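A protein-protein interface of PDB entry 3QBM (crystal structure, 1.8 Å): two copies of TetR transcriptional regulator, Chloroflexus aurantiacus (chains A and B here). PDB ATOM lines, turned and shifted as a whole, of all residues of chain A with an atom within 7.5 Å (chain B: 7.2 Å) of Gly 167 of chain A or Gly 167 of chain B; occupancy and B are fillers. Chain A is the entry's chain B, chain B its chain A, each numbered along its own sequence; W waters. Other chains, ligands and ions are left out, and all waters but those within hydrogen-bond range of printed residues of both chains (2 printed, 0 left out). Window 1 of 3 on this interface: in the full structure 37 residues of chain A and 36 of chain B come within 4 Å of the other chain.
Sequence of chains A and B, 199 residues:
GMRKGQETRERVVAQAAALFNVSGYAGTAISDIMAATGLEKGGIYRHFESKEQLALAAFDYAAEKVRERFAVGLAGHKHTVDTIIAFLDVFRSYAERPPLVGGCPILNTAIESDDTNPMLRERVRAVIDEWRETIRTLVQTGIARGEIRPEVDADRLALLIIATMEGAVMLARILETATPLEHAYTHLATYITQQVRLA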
ATOM      1  N   PHE A  91     -16.698 -16.450 -18.487  1.00  0.00           N
ATOM      2  CA  PHE A  91     -16.796 -16.339 -19.935  1.00  0.00           C
ATOM      3  C   PHE A  91     -18.225 -16.607 -20.398  1.00  0.00           C
ATOM      4  O   PHE A  91     -18.745 -15.921 -21.299  1.00  0.00           O
ATOM      5  CB  PHE A  91     -15.853 -17.353 -20.585  1.00  0.00           C
ATOM      6  CG  PHE A  91     -14.436 -16.911 -20.637  1.00  0.00           C
ATOM      7  CD1 PHE A  91     -14.058 -15.913 -21.512  1.00  0.00           C
ATOM      8  CD2 PHE A  91     -13.455 -17.531 -19.881  1.00  0.00           C
ATOM      9  CE1 PHE A  91     -12.720 -15.541 -21.616  1.00  0.00           C
ATOM     10  CE2 PHE A  91     -12.151 -17.163 -20.012  1.00  0.00           C
ATOM     11  CZ  PHE A  91     -11.794 -16.153 -20.857  1.00  0.00           C
ATOM     12  N   LEU A 107      -9.745 -10.988 -26.520  1.00  0.00           N
ATOM     13  CA  LEU A 107     -10.003 -11.595 -27.840  1.00  0.00           C
ATOM     14  C   LEU A 107      -9.977 -10.516 -28.924  1.00  0.00           C
ATOM     15  O   LEU A 107      -9.329 -10.691 -29.951  1.00  0.00           O
ATOM     16  CB  LEU A 107     -11.393 -12.279 -27.843  1.00  0.00           C
ATOM     17  CG  LEU A 107     -11.989 -12.697 -29.175  1.00  0.00           C
ATOM     18  CD1 LEU A 107     -11.064 -13.683 -29.895  1.00  0.00           C
ATOM     19  CD2 LEU A 107     -13.393 -13.282 -28.929  1.00  0.00           C
ATOM     20  N   LEU A 159      -4.758 -23.667 -21.471  1.00  0.00           N
ATOM     21  CA  LEU A 159      -4.802 -23.288 -22.908  1.00  0.00           C
ATOM     22  C   LEU A 159      -6.090 -23.808 -23.549  1.00  0.00           C
ATOM     23  O   LEU A 159      -6.705 -23.093 -24.359  1.00  0.00           O
ATOM     24  CB  LEU A 159      -3.571 -23.802 -23.651  1.00  0.00           C
ATOM     25  CG  LEU A 159      -2.223 -23.120 -23.335  1.00  0.00           C
ATOM     26  CD1 LEU A 159      -1.078 -23.796 -24.047  1.00  0.00           C
ATOM     27  CD2 LEU A 159      -2.267 -21.671 -23.712  1.00  0.00           C
ATOM     28  N   LEU A 160      -6.498 -25.020 -23.191  1.00  0.00           N
ATOM     29  CA  LEU A 160      -7.794 -25.560 -23.689  1.00  0.00           C
ATOM     30  C   LEU A 160      -8.999 -24.701 -23.237  1.00  0.00           C
ATOM     31  O   LEU A 160      -9.829 -24.333 -24.052  1.00  0.00           O
ATOM     32  CB  LEU A 160      -8.000 -27.010 -23.282  1.00  0.00           C
ATOM     33  CG  LEU A 160      -9.312 -27.686 -23.697  1.00  0.00           C
ATOM     34  CD1 LEU A 160      -9.401 -27.758 -25.205  1.00  0.00           C
ATOM     35  CD2 LEU A 160      -9.451 -29.091 -23.037  1.00  0.00           C
ATOM     36  N   ILE A 161      -9.053 -24.361 -21.957  1.00  0.00           N
ATOM     37  CA  ILE A 161     -10.149 -23.517 -21.422  1.00  0.00           C
ATOM     38  C   ILE A 161     -10.206 -22.157 -22.151  1.00  0.00           C
ATOM     39  O   ILE A 161     -11.279 -21.719 -22.652  1.00  0.00           O
ATOM     40  CB  ILE A 161      -9.943 -23.281 -19.900  1.00  0.00           C
ATOM     41  CG1 ILE A 161     -10.184 -24.574 -19.149  1.00  0.00           C
ATOM     42  CG2 ILE A 161     -10.873 -22.133 -19.409  1.00  0.00           C
ATOM     43  CD1 ILE A 161      -9.804 -24.532 -17.686  1.00  0.00           C
ATOM     44  N   ILE A 162      -9.036 -21.514 -22.269  1.00  0.00           N
ATOM     45  CA  ILE A 162      -8.982 -20.187 -22.872  1.00  0.00           C
ATOM     46  C   ILE A 162      -9.404 -20.276 -24.346  1.00  0.00           C
ATOM     47  O   ILE A 162     -10.213 -19.499 -24.778  1.00  0.00           O
ATOM     48  CB  ILE A 162      -7.602 -19.507 -22.668  1.00  0.00           C
ATOM     49  CG1 ILE A 162      -7.359 -19.298 -21.172  1.00  0.00           C
ATOM     50  CG2 ILE A 162      -7.472 -18.141 -23.470  1.00  0.00           C
ATOM     51  CD1 ILE A 162      -5.852 -19.176 -20.771  1.00  0.00           C
ATOM     52  N   ALA A 163      -8.888 -21.253 -25.098  1.00  0.00           N
ATOM     53  CA  ALA A 163      -9.226 -21.370 -26.515  1.00  0.00           C
ATOM     54  C   ALA A 163     -10.724 -21.612 -26.710  1.00  0.00           C
ATOM     55  O   ALA A 163     -11.399 -20.915 -27.497  1.00  0.00           O
ATOM     56  CB  ALA A 163      -8.408 -22.486 -27.178  1.00  0.00           C
ATOM     57  N   THR A 164     -11.247 -22.576 -25.978  1.00  0.00           N
ATOM     58  CA  THR A 164     -12.654 -22.947 -26.089  1.00  0.00           C
ATOM     59  C   THR A 164     -13.588 -21.819 -25.719  1.00  0.00           C
ATOM     60  O   THR A 164     -14.506 -21.530 -26.449  1.00  0.00           O
ATOM     61  CB  THR A 164     -12.976 -24.220 -25.248  1.00  0.00           C
ATOM     62  OG1 THR A 164     -12.048 -25.290 -25.571  1.00  0.00           O
ATOM     63  CG2 THR A 164     -14.403 -24.677 -25.487  1.00  0.00           C
ATOM     64  N   MET A 165     -13.359 -21.169 -24.582  1.00  0.00           N
ATOM     65  CA  MET A 165     -14.287 -20.162 -24.139  1.00  0.00           C
ATOM     66  C   MET A 165     -14.199 -18.938 -25.030  1.00  0.00           C
ATOM     67  O   MET A 165     -15.264 -18.387 -25.371  1.00  0.00           O
ATOM     68  CB  MET A 165     -14.073 -19.824 -22.657  1.00  0.00           C
ATOM     69  CG  MET A 165     -14.327 -21.043 -21.708  1.00  0.00           C
ATOM     70  SD  MET A 165     -16.010 -21.999 -21.956  1.00  0.00           S
ATOM     71  CE  MET A 165     -17.327 -20.645 -21.646  1.00  0.00           C
ATOM     72  N   GLU A 166     -12.986 -18.523 -25.429  1.00  0.00           N
ATOM     73  CA  GLU A 166     -12.865 -17.360 -26.313  1.00  0.00           C
ATOM     74  C   GLU A 166     -13.424 -17.609 -27.681  1.00  0.00           C
ATOM     75  O   GLU A 166     -14.031 -16.721 -28.260  1.00  0.00           O
ATOM     76  CB  GLU A 166     -11.415 -16.835 -26.402  1.00  0.00           C
ATOM     77  CG  GLU A 166     -10.915 -16.166 -25.085  1.00  0.00           C
ATOM     78  CD  GLU A 166     -11.560 -14.784 -24.840  1.00  0.00           C
ATOM     79  OE1 GLU A 166     -12.728 -14.529 -25.260  1.00  0.00           O
ATOM     80  OE2 GLU A 166     -10.872 -13.940 -24.269  1.00  0.00           O
ATOM     81  N   GLY A 167     -13.200 -18.802 -28.245  1.00  0.00           N
ATOM     82  CA  GLY A 167     -13.825 -19.115 -29.523  1.00  0.00           C
ATOM     83  C   GLY A 167     -15.363 -19.062 -29.452  1.00  0.00           C
ATOM     84  O   GLY A 167     -16.045 -18.637 -30.402  1.00  0.00           O
ATOM     85  N   ALA A 168     -15.908 -19.519 -28.328  1.00  0.00           N
ATOM     86  CA  ALA A 168     -17.352 -19.475 -28.087  1.00  0.00           C
ATOM     87  C   ALA A 168     -17.851 -18.049 -27.936  1.00  0.00           C
ATOM     88  O   ALA A 168     -18.953 -17.723 -28.394  1.00  0.00           O
ATOM     89  CB  ALA A 168     -17.700 -20.335 -26.883  1.00  0.00           C
ATOM     90  N   VAL A 169     -17.055 -17.189 -27.301  1.00  0.00           N
ATOM     91  CA  VAL A 169     -17.391 -15.748 -27.233  1.00  0.00           C
ATOM     92  C   VAL A 169     -17.470 -15.174 -28.642  1.00  0.00           C
ATOM     93  O   VAL A 169     -18.398 -14.429 -28.944  1.00  0.00           O
ATOM     94  CB  VAL A 169     -16.353 -14.922 -26.394  1.00  0.00           C
ATOM     95  CG1 VAL A 169     -16.452 -13.427 -26.668  1.00  0.00           C
ATOM     96  CG2 VAL A 169     -16.470 -15.264 -24.879  1.00  0.00           C
ATOM     97  N   MET A 170     -16.500 -15.495 -29.502  1.00  0.00           N
ATOM     98  CA  MET A 170     -16.561 -15.095 -30.907  1.00  0.00           C
ATOM     99  C   MET A 170     -17.856 -15.565 -31.571  1.00  0.00           C
ATOM    100  O   MET A 170     -18.583 -14.772 -32.224  1.00  0.00           O
ATOM    101  CB  MET A 170     -15.371 -15.656 -31.692  1.00  0.00           C
ATOM    102  CG  MET A 170     -15.346 -15.277 -33.171  1.00  0.00           C
ATOM    103  SD  MET A 170     -16.316 -16.322 -34.326  1.00  0.00           S
ATOM    104  CE  MET A 170     -15.343 -18.026 -34.116  1.00  0.00           C
ATOM    105  N   LEU A 171     -18.168 -16.850 -31.408  1.00  0.00           N
ATOM    106  CA  LEU A 171     -19.345 -17.407 -32.055  1.00  0.00           C
ATOM    107  C   LEU A 171     -20.657 -16.789 -31.569  1.00  0.00           C
ATOM    108  O   LEU A 171     -21.573 -16.562 -32.368  1.00  0.00           O
ATOM    109  CB  LEU A 171     -19.412 -18.932 -31.896  1.00  0.00           C
ATOM    110  CG  LEU A 171     -18.513 -19.818 -32.727  1.00  0.00           C
ATOM    111  CD1 LEU A 171     -18.774 -21.302 -32.354  1.00  0.00           C
ATOM    112  CD2 LEU A 171     -18.692 -19.606 -34.267  1.00  0.00           C
ATOM    113  N   ALA A 172     -20.733 -16.526 -30.268  1.00  0.00           N
ATOM    114  CA  ALA A 172     -21.966 -16.010 -29.659  1.00  0.00           C
ATOM    115  C   ALA A 172     -22.333 -14.632 -30.175  1.00  0.00           C
ATOM    116  O   ALA A 172     -23.521 -14.323 -30.316  1.00  0.00           O
ATOM    117  CB  ALA A 172     -21.837 -16.013 -28.139  1.00  0.00           C
ATOM    118  N   ARG A 173     -21.345 -13.794 -30.485  1.00  0.00           N
ATOM    119  CA  ARG A 173     -21.636 -12.451 -31.034  1.00  0.00           C
ATOM    120  C   ARG A 173     -21.935 -12.475 -32.530  1.00  0.00           C
ATOM    121  O   ARG A 173     -22.586 -11.577 -33.055  1.00  0.00           O
ATOM    122  CB  ARG A 173     -20.502 -11.469 -30.754  1.00  0.00           C
ATOM    123  CG  ARG A 173     -20.177 -11.242 -29.260  1.00  0.00           C
ATOM    124  CD  ARG A 173     -19.349  -9.928 -29.019  1.00  0.00           C
ATOM    125  NE  ARG A 173     -20.182  -8.740 -29.131  1.00  0.00           N
ATOM    126  CZ  ARG A 173     -21.026  -8.295 -28.210  1.00  0.00           C
ATOM    127  NH1 ARG A 173     -21.197  -8.947 -27.084  1.00  0.00           N
ATOM    128  NH2 ARG A 173     -21.746  -7.196 -28.440  1.00  0.00           N
ATOM    129  N   PRO A 180     -23.541 -21.035 -28.190  1.00  0.00           N
ATOM    130  CA  PRO A 180     -22.154 -21.553 -28.239  1.00  0.00           C
ATOM    131  C   PRO A 180     -21.439 -21.503 -26.897  1.00  0.00           C
ATOM    132  O   PRO A 180     -20.683 -22.421 -26.551  1.00  0.00           O
ATOM    133  CB  PRO A 180     -21.474 -20.602 -29.220  1.00  0.00           C
ATOM    134  CG  PRO A 180     -22.547 -20.002 -29.983  1.00  0.00           C
ATOM    135  CD  PRO A 180     -23.699 -19.889 -29.081  1.00  0.00           C
ATOM    136  N   LEU A 181     -21.713 -20.458 -26.126  1.00  0.00           N
ATOM    137  CA  LEU A 181     -21.092 -20.294 -24.794  1.00  0.00           C
ATOM    138  C   LEU A 181     -21.646 -21.314 -23.797  1.00  0.00           C
ATOM    139  O   LEU A 181     -20.898 -21.923 -23.024  1.00  0.00           O
ATOM    140  CB  LEU A 181     -21.244 -18.838 -24.322  1.00  0.00           C
ATOM    141  CG  LEU A 181     -20.132 -17.909 -24.800  1.00  0.00           C
ATOM    142  CD1 LEU A 181     -20.511 -16.434 -24.583  1.00  0.00           C
ATOM    143  CD2 LEU A 181     -18.804 -18.212 -24.113  1.00  0.00           C
ATOM    144  N   ALA A 184     -20.030 -24.697 -24.801  1.00  0.00           N
ATOM    145  CA  ALA A 184     -18.606 -24.729 -24.481  1.00  0.00           C
ATOM    146  C   ALA A 184     -18.435 -24.889 -22.961  1.00  0.00           C
ATOM    147  O   ALA A 184     -17.637 -25.704 -22.500  1.00  0.00           O
ATOM    148  CB  ALA A 184     -17.870 -23.435 -25.014  1.00  0.00           C
ATOM    149  N   PHE B  91      -7.856 -26.956 -39.238  1.00  0.00           N
ATOM    150  CA  PHE B  91      -7.553 -25.865 -38.316  1.00  0.00           C
ATOM    151  C   PHE B  91      -6.146 -25.979 -37.710  1.00  0.00           C
ATOM    152  O   PHE B  91      -5.419 -24.980 -37.620  1.00  0.00           O
ATOM    153  CB  PHE B  91      -8.597 -25.815 -37.206  1.00  0.00           C
ATOM    154  CG  PHE B  91      -9.846 -25.090 -37.590  1.00  0.00           C
ATOM    155  CD1 PHE B  91      -9.839 -23.713 -37.674  1.00  0.00           C
ATOM    156  CD2 PHE B  91     -11.023 -25.758 -37.826  1.00  0.00           C
ATOM    157  CE1 PHE B  91     -10.978 -23.023 -37.977  1.00  0.00           C
ATOM    158  CE2 PHE B  91     -12.173 -25.051 -38.101  1.00  0.00           C
ATOM    159  CZ  PHE B  91     -12.144 -23.705 -38.206  1.00  0.00           C
ATOM    160  N   LEU B 107     -12.560 -15.884 -38.454  1.00  0.00           N
ATOM    161  CA  LEU B 107     -12.278 -15.365 -37.120  1.00  0.00           C
ATOM    162  C   LEU B 107     -11.966 -13.869 -37.172  1.00  0.00           C
ATOM    163  O   LEU B 107     -12.537 -13.070 -36.416  1.00  0.00           O
ATOM    164  CB  LEU B 107     -11.108 -16.127 -36.478  1.00  0.00           C
ATOM    165  CG  LEU B 107     -10.496 -15.660 -35.157  1.00  0.00           C
ATOM    166  CD1 LEU B 107     -11.535 -15.680 -34.032  1.00  0.00           C
ATOM    167  CD2 LEU B 107      -9.219 -16.462 -34.770  1.00  0.00           C
ATOM    168  N   LEU B 159     -20.690 -26.693 -33.007  1.00  0.00           N
ATOM    169  CA  LEU B 159     -20.362 -25.438 -32.365  1.00  0.00           C
ATOM    170  C   LEU B 159     -19.214 -25.605 -31.373  1.00  0.00           C
ATOM    171  O   LEU B 159     -18.398 -24.703 -31.251  1.00  0.00           O
ATOM    172  CB  LEU B 159     -21.581 -24.846 -31.684  1.00  0.00           C
ATOM    173  CG  LEU B 159     -22.731 -24.401 -32.551  1.00  0.00           C
ATOM    174  CD1 LEU B 159     -23.941 -24.110 -31.650  1.00  0.00           C
ATOM    175  CD2 LEU B 159     -22.428 -23.185 -33.350  1.00  0.00           C
ATOM    176  N   ILE B 161     -16.635 -27.773 -31.649  1.00  0.00           N
ATOM    177  CA  ILE B 161     -15.493 -27.885 -32.533  1.00  0.00           C
ATOM    178  C   ILE B 161     -15.082 -26.521 -33.079  1.00  0.00           C
ATOM    179  O   ILE B 161     -13.930 -26.158 -32.998  1.00  0.00           O
ATOM    180  CB  ILE B 161     -15.792 -28.810 -33.732  1.00  0.00           C
ATOM    181  CG1 ILE B 161     -15.739 -30.265 -33.293  1.00  0.00           C
ATOM    182  CG2 ILE B 161     -14.797 -28.518 -34.872  1.00  0.00           C
ATOM    183  CD1 ILE B 161     -16.366 -31.253 -34.354  1.00  0.00           C
ATOM    184  N   ILE B 162     -16.028 -25.759 -33.629  1.00  0.00           N
ATOM    185  CA  ILE B 162     -15.703 -24.450 -34.203  1.00  0.00           C
ATOM    186  C   ILE B 162     -15.147 -23.462 -33.179  1.00  0.00           C
ATOM    187  O   ILE B 162     -14.146 -22.784 -33.443  1.00  0.00           O
ATOM    188  CB  ILE B 162     -16.919 -23.832 -34.941  1.00  0.00           C
ATOM    189  CG1 ILE B 162     -17.296 -24.731 -36.106  1.00  0.00           C
ATOM    190  CG2 ILE B 162     -16.613 -22.381 -35.410  1.00  0.00           C
ATOM    191  CD1 ILE B 162     -18.746 -24.433 -36.680  1.00  0.00           C
ATOM    192  N   ALA B 163     -15.785 -23.417 -32.019  1.00  0.00           N
ATOM    193  CA  ALA B 163     -15.363 -22.542 -30.913  1.00  0.00           C
ATOM    194  C   ALA B 163     -13.953 -22.924 -30.503  1.00  0.00           C
ATOM    195  O   ALA B 163     -13.063 -22.051 -30.396  1.00  0.00           O
ATOM    196  CB  ALA B 163     -16.301 -22.668 -29.683  1.00  0.00           C
ATOM    197  N   THR B 164     -13.732 -24.210 -30.257  1.00  0.00           N
ATOM    198  CA  THR B 164     -12.418 -24.660 -29.779  1.00  0.00           C
ATOM    199  C   THR B 164     -11.294 -24.360 -30.732  1.00  0.00           C
ATOM    200  O   THR B 164     -10.225 -23.831 -30.315  1.00  0.00           O
ATOM    201  CB  THR B 164     -12.446 -26.158 -29.476  1.00  0.00           C
ATOM    202  OG1 THR B 164     -13.508 -26.405 -28.531  1.00  0.00           O
ATOM    203  CG2 THR B 164     -11.101 -26.630 -28.866  1.00  0.00           C
ATOM    204  N   MET B 165     -11.505 -24.725 -31.987  1.00  0.00           N
ATOM    205  CA  MET B 165     -10.463 -24.605 -33.000  1.00  0.00           C
ATOM    206  C   MET B 165     -10.195 -23.134 -33.326  1.00  0.00           C
ATOM    207  O   MET B 165      -9.034 -22.730 -33.409  1.00  0.00           O
ATOM    208  CB  MET B 165     -10.769 -25.443 -34.251  1.00  0.00           C
ATOM    209  CG  MET B 165     -10.792 -26.953 -34.028  1.00  0.00           C
ATOM    210  SD  MET B 165      -9.412 -27.751 -32.867  1.00  0.00           S
ATOM    211  CE  MET B 165      -7.831 -27.426 -33.961  1.00  0.00           C
ATOM    212  N   GLU B 166     -11.234 -22.308 -33.441  1.00  0.00           N
ATOM    213  CA  GLU B 166     -11.034 -20.902 -33.732  1.00  0.00           C
ATOM    214  C   GLU B 166     -10.369 -20.188 -32.561  1.00  0.00           C
ATOM    215  O   GLU B 166      -9.492 -19.351 -32.793  1.00  0.00           O
ATOM    216  CB  GLU B 166     -12.347 -20.191 -34.101  1.00  0.00           C
ATOM    217  CG  GLU B 166     -12.878 -20.537 -35.462  1.00  0.00           C
ATOM    218  CD  GLU B 166     -12.108 -19.906 -36.605  1.00  0.00           C
ATOM    219  OE1 GLU B 166     -10.881 -19.681 -36.499  1.00  0.00           O
ATOM    220  OE2 GLU B 166     -12.757 -19.630 -37.614  1.00  0.00           O
ATOM    221  N   GLY B 167     -10.777 -20.495 -31.317  1.00  0.00           N
ATOM    222  CA  GLY B 167     -10.089 -19.963 -30.120  1.00  0.00           C
ATOM    223  C   GLY B 167      -8.595 -20.349 -30.063  1.00  0.00           C
ATOM    224  O   GLY B 167      -7.709 -19.550 -29.727  1.00  0.00           O
ATOM    225  N   ALA B 168      -8.305 -21.567 -30.477  1.00  0.00           N
ATOM    226  CA  ALA B 168      -6.925 -22.013 -30.546  1.00  0.00           C
ATOM    227  C   ALA B 168      -6.129 -21.300 -31.645  1.00  0.00           C
ATOM    228  O   ALA B 168      -4.955 -21.010 -31.447  1.00  0.00           O
ATOM    229  CB  ALA B 168      -6.888 -23.493 -30.697  1.00  0.00           C
ATOM    230  N   VAL B 169      -6.756 -21.022 -32.786  1.00  0.00           N
ATOM    231  CA  VAL B 169      -6.149 -20.194 -33.856  1.00  0.00           C
ATOM    232  C   VAL B 169      -5.760 -18.819 -33.284  1.00  0.00           C
ATOM    233  O   VAL B 169      -4.612 -18.360 -33.469  1.00  0.00           O
ATOM    234  CB  VAL B 169      -7.064 -20.006 -35.059  1.00  0.00           C
ATOM    235  CG1 VAL B 169      -6.488 -18.942 -36.013  1.00  0.00           C
ATOM    236  CG2 VAL B 169      -7.230 -21.321 -35.808  1.00  0.00           C
ATOM    237  N   MET B 170      -6.679 -18.195 -32.549  1.00  0.00           N
ATOM    238  CA  MET B 170      -6.420 -16.924 -31.879  1.00  0.00           C
ATOM    239  C   MET B 170      -5.226 -17.029 -30.902  1.00  0.00           C
ATOM    240  O   MET B 170      -4.307 -16.212 -30.930  1.00  0.00           O
ATOM    241  CB  MET B 170      -7.652 -16.489 -31.092  1.00  0.00           C
ATOM    242  CG  MET B 170      -7.458 -15.145 -30.331  1.00  0.00           C
ATOM    243  SD  MET B 170      -6.662 -15.218 -28.643  1.00  0.00           S
ATOM    244  CE  MET B 170      -8.104 -16.266 -27.779  1.00  0.00           C
ATOM    245  N   LEU B 171      -5.260 -18.043 -30.048  1.00  0.00           N
ATOM    246  CA  LEU B 171      -4.203 -18.232 -29.029  1.00  0.00           C
ATOM    247  C   LEU B 171      -2.848 -18.550 -29.609  1.00  0.00           C
ATOM    248  O   LEU B 171      -1.845 -18.042 -29.133  1.00  0.00           O
ATOM    249  CB  LEU B 171      -4.519 -19.379 -28.105  1.00  0.00           C
ATOM    250  CG  LEU B 171      -5.454 -19.088 -26.959  1.00  0.00           C
ATOM    251  CD1 LEU B 171      -5.594 -20.407 -26.221  1.00  0.00           C
ATOM    252  CD2 LEU B 171      -4.960 -17.944 -26.042  1.00  0.00           C
ATOM    253  N   ALA B 172      -2.827 -19.393 -30.642  1.00  0.00           N
ATOM    254  CA  ALA B 172      -1.574 -19.796 -31.276  1.00  0.00           C
ATOM    255  C   ALA B 172      -0.912 -18.580 -31.895  1.00  0.00           C
ATOM    256  O   ALA B 172       0.300 -18.422 -31.796  1.00  0.00           O
ATOM    257  CB  ALA B 172      -1.807 -20.904 -32.309  1.00  0.00           C
ATOM    258  N   ARG B 173      -1.691 -17.680 -32.482  1.00  0.00           N
ATOM    259  CA  ARG B 173      -1.093 -16.521 -33.125  1.00  0.00           C
ATOM    260  C   ARG B 173      -0.580 -15.536 -32.102  1.00  0.00           C
ATOM    261  O   ARG B 173       0.548 -15.043 -32.214  1.00  0.00           O
ATOM    262  CB  ARG B 173      -2.026 -15.837 -34.111  1.00  0.00           C
ATOM    263  CG  ARG B 173      -2.293 -16.575 -35.399  1.00  0.00           C
ATOM    264  CD  ARG B 173      -2.898 -15.627 -36.505  1.00  0.00           C
ATOM    265  NE  ARG B 173      -1.927 -14.807 -37.208  1.00  0.00           N
ATOM    266  CZ  ARG B 173      -1.091 -15.275 -38.130  1.00  0.00           C
ATOM    267  NH1 ARG B 173      -1.065 -16.573 -38.420  1.00  0.00           N
ATOM    268  NH2 ARG B 173      -0.233 -14.477 -38.734  1.00  0.00           N
ATOM    269  N   ILE B 174      -1.366 -15.292 -31.058  1.00  0.00           N
ATOM    270  CA  ILE B 174      -0.954 -14.325 -30.062  1.00  0.00           C
ATOM    271  C   ILE B 174       0.213 -14.818 -29.168  1.00  0.00           C
ATOM    272  O   ILE B 174       1.121 -14.026 -28.832  1.00  0.00           O
ATOM    273  CB  ILE B 174      -2.230 -13.749 -29.307  1.00  0.00           C
ATOM    274  CG1 ILE B 174      -1.990 -12.322 -28.821  1.00  0.00           C
ATOM    275  CG2 ILE B 174      -2.692 -14.737 -28.221  1.00  0.00           C
ATOM    276  CD1 ILE B 174      -1.830 -11.239 -29.942  1.00  0.00           C
ATOM    277  N   PRO B 180      -1.221 -24.277 -28.603  1.00  0.00           N
ATOM    278  CA  PRO B 180      -2.676 -24.259 -28.388  1.00  0.00           C
ATOM    279  C   PRO B 180      -3.501 -25.026 -29.449  1.00  0.00           C
ATOM    280  O   PRO B 180      -4.526 -25.629 -29.135  1.00  0.00           O
ATOM    281  CB  PRO B 180      -3.030 -22.751 -28.438  1.00  0.00           C
ATOM    282  CG  PRO B 180      -1.771 -22.053 -28.043  1.00  0.00           C
ATOM    283  CD  PRO B 180      -0.659 -22.902 -28.638  1.00  0.00           C
ATOM    284  N   LEU B 181      -3.070 -24.974 -30.703  1.00  0.00           N
ATOM    285  CA  LEU B 181      -3.747 -25.710 -31.753  1.00  0.00           C
ATOM    286  C   LEU B 181      -3.531 -27.219 -31.596  1.00  0.00           C
ATOM    287  O   LEU B 181      -4.426 -28.008 -31.860  1.00  0.00           O
ATOM    288  CB  LEU B 181      -3.293 -25.210 -33.147  1.00  0.00           C
ATOM    289  CG  LEU B 181      -4.021 -23.970 -33.660  1.00  0.00           C
ATOM    290  CD1 LEU B 181      -3.273 -23.306 -34.817  1.00  0.00           C
ATOM    291  CD2 LEU B 181      -5.448 -24.300 -34.105  1.00  0.00           C
ATOM    292  N   ALA B 184      -5.752 -28.357 -28.600  1.00  0.00           N
ATOM    293  CA  ALA B 184      -7.161 -28.331 -28.992  1.00  0.00           C
ATOM    294  C   ALA B 184      -7.449 -29.510 -29.894  1.00  0.00           C
ATOM    295  O   ALA B 184      -8.415 -30.257 -29.677  1.00  0.00           O
ATOM    296  CB  ALA B 184      -7.481 -27.020 -29.690  1.00  0.00           C
HETATM  297  O   HOH W   1      -5.705 -25.260 -26.437  1.00  0.00           O
HETATM  298  O   HOH W   2     -12.885 -27.906 -26.149  1.00  0.00           O
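The side-chain hydroxyl (OG1) of Thr 164 of chain B is in hydrogen-bond range of the side-chain hydroxyl (OG1) of Thr 164 of chain A (3.5 Å).
OG1 of Thr 164 of chain A is in hydrogen-bond range of O of Leu 160 of chain A (2.9 Å).
Among the printed residues, merely in contact across the chains: Leu 107 of chain A with Met 170 of chain B (3.9 Å), Leu 159 of chain A with Leu 171 of chain B (3.5 Å), Ile 162 of chain A with Leu 171 of chain B (3.6 Å), Ala 163 of chain A with Ala 163 of chain B (3.5 Å), Ala 163 of chain A with Thr 164 of chain B (3.9 Å), Ala 163 of chain A with Gly 167 of chain B (3.1 Å), Ala 163 of chain A with Ala 168 of chain B (3.4 Å), Ala 163 of chain A with Leu 171 of chain B (3.6 Å), Thr 164 of chain A with Ala 163 of chain B (3.9 Å), Glu 166 of chain A with Met 170 of chain B (3.6 Å), Gly 167 of chain A with Ala 163 of chain B (3.2 Å), Gly 167 of chain A with Gly 167 of chain B (3.8 Å), Ala 168 of chain A with Ala 163 of chain B (3.5 Å), Met 170 of chain A with Leu 107 of chain B (3.9 Å), Met 170 of chain A with Glu 166 of chain B (3.7 Å), Leu 171 of chain A with Leu 159 of chain B (3.6 Å), Leu 171 of chain A with Ile 162 of chain B (3.7 Å) and Leu 171 of chain A with Ala 163 of chain B (3.7 Å).
Printed residues of chain B within 4 Å of Leu 159 of chain A: Leu 171 (3.5 Å).
Leu 160 of chain A touches none of the printed residues of chain B.
Printed residues of chain B within 4 Å of Ala 163 of chain A: Ala 163 (3.5 Å), Thr 164 (3.9 Å), Gly 167 (3.1 Å), Ala 168 (3.4 Å) and Leu 171 (3.6 Å).
Of the printed residues of chain B, Gly 167 of chain A touches Ala 163 and Gly 167.
Printed residues of chain B within 4 Å of Ala 168 of chain A: Ala 163.
Printed residues of chain A within 4 Å of Glu 166 of chain B: Met 170.
Gly 167 of chain B touches just these residues of chain A: Ala 163 and Gly 167.
The nearest residue of chain B that does not touch Gly 167 of chain A is Glu 166 of chain B (4.7 Å).
The nearest residue of chain A that does not touch Gly 167 of chain B is Glu 166 of chain A (4.8 Å).
Of the 20 printed residues of chain B, 10 touch a printed residue of chain A.
Hydrophobic or aromatic side chains of chain B that line the printed part of chain A: Leu 107, Ile 162, Ala 163, Ala 168, Met 170 and Leu 171.
Among the printed residues, 19 pairs touch across the chains.
Ala 163 of chain B touches its own counterpart, Ala 163 of chain A.
Ala 163 of chain A touches Ala 168 of chain B, and with the chains exchanged Ala 168 of chain A touches Ala 163 of chain B.
Glu 166 of chain A touches Met 170 of chain B, and with the chains exchanged Met 170 of chain A touches Glu 166 of chain B.
Gly 167 of chain A touches its own counterpart, Gly 167 of chain B.
Positions printed for both chains: 91, 107, 159, 161, 162, 163, 164, 165, 166, 167, 168, 169, 170, 171, 172, 173, 180, 181 and 184.
Of the 19 pairs that touch across the chains among the printed residues, 19 have their exchanged pair printed and touching as well.
Water W2 lies within hydrogen-bond range of the side-chain hydroxyl (OG1) of Thr 164 of chain A (2.8 Å) and the side-chain hydroxyl (OG1) of Thr 164 of chain B (2.9 Å).
Water W1 lies within hydrogen-bond range of the backbone carbonyl oxygen of Pro 180 of chain B, the backbone carbonyl oxygen of Leu 159 of chain A and the backbone NH of Leu 160 of chain A.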
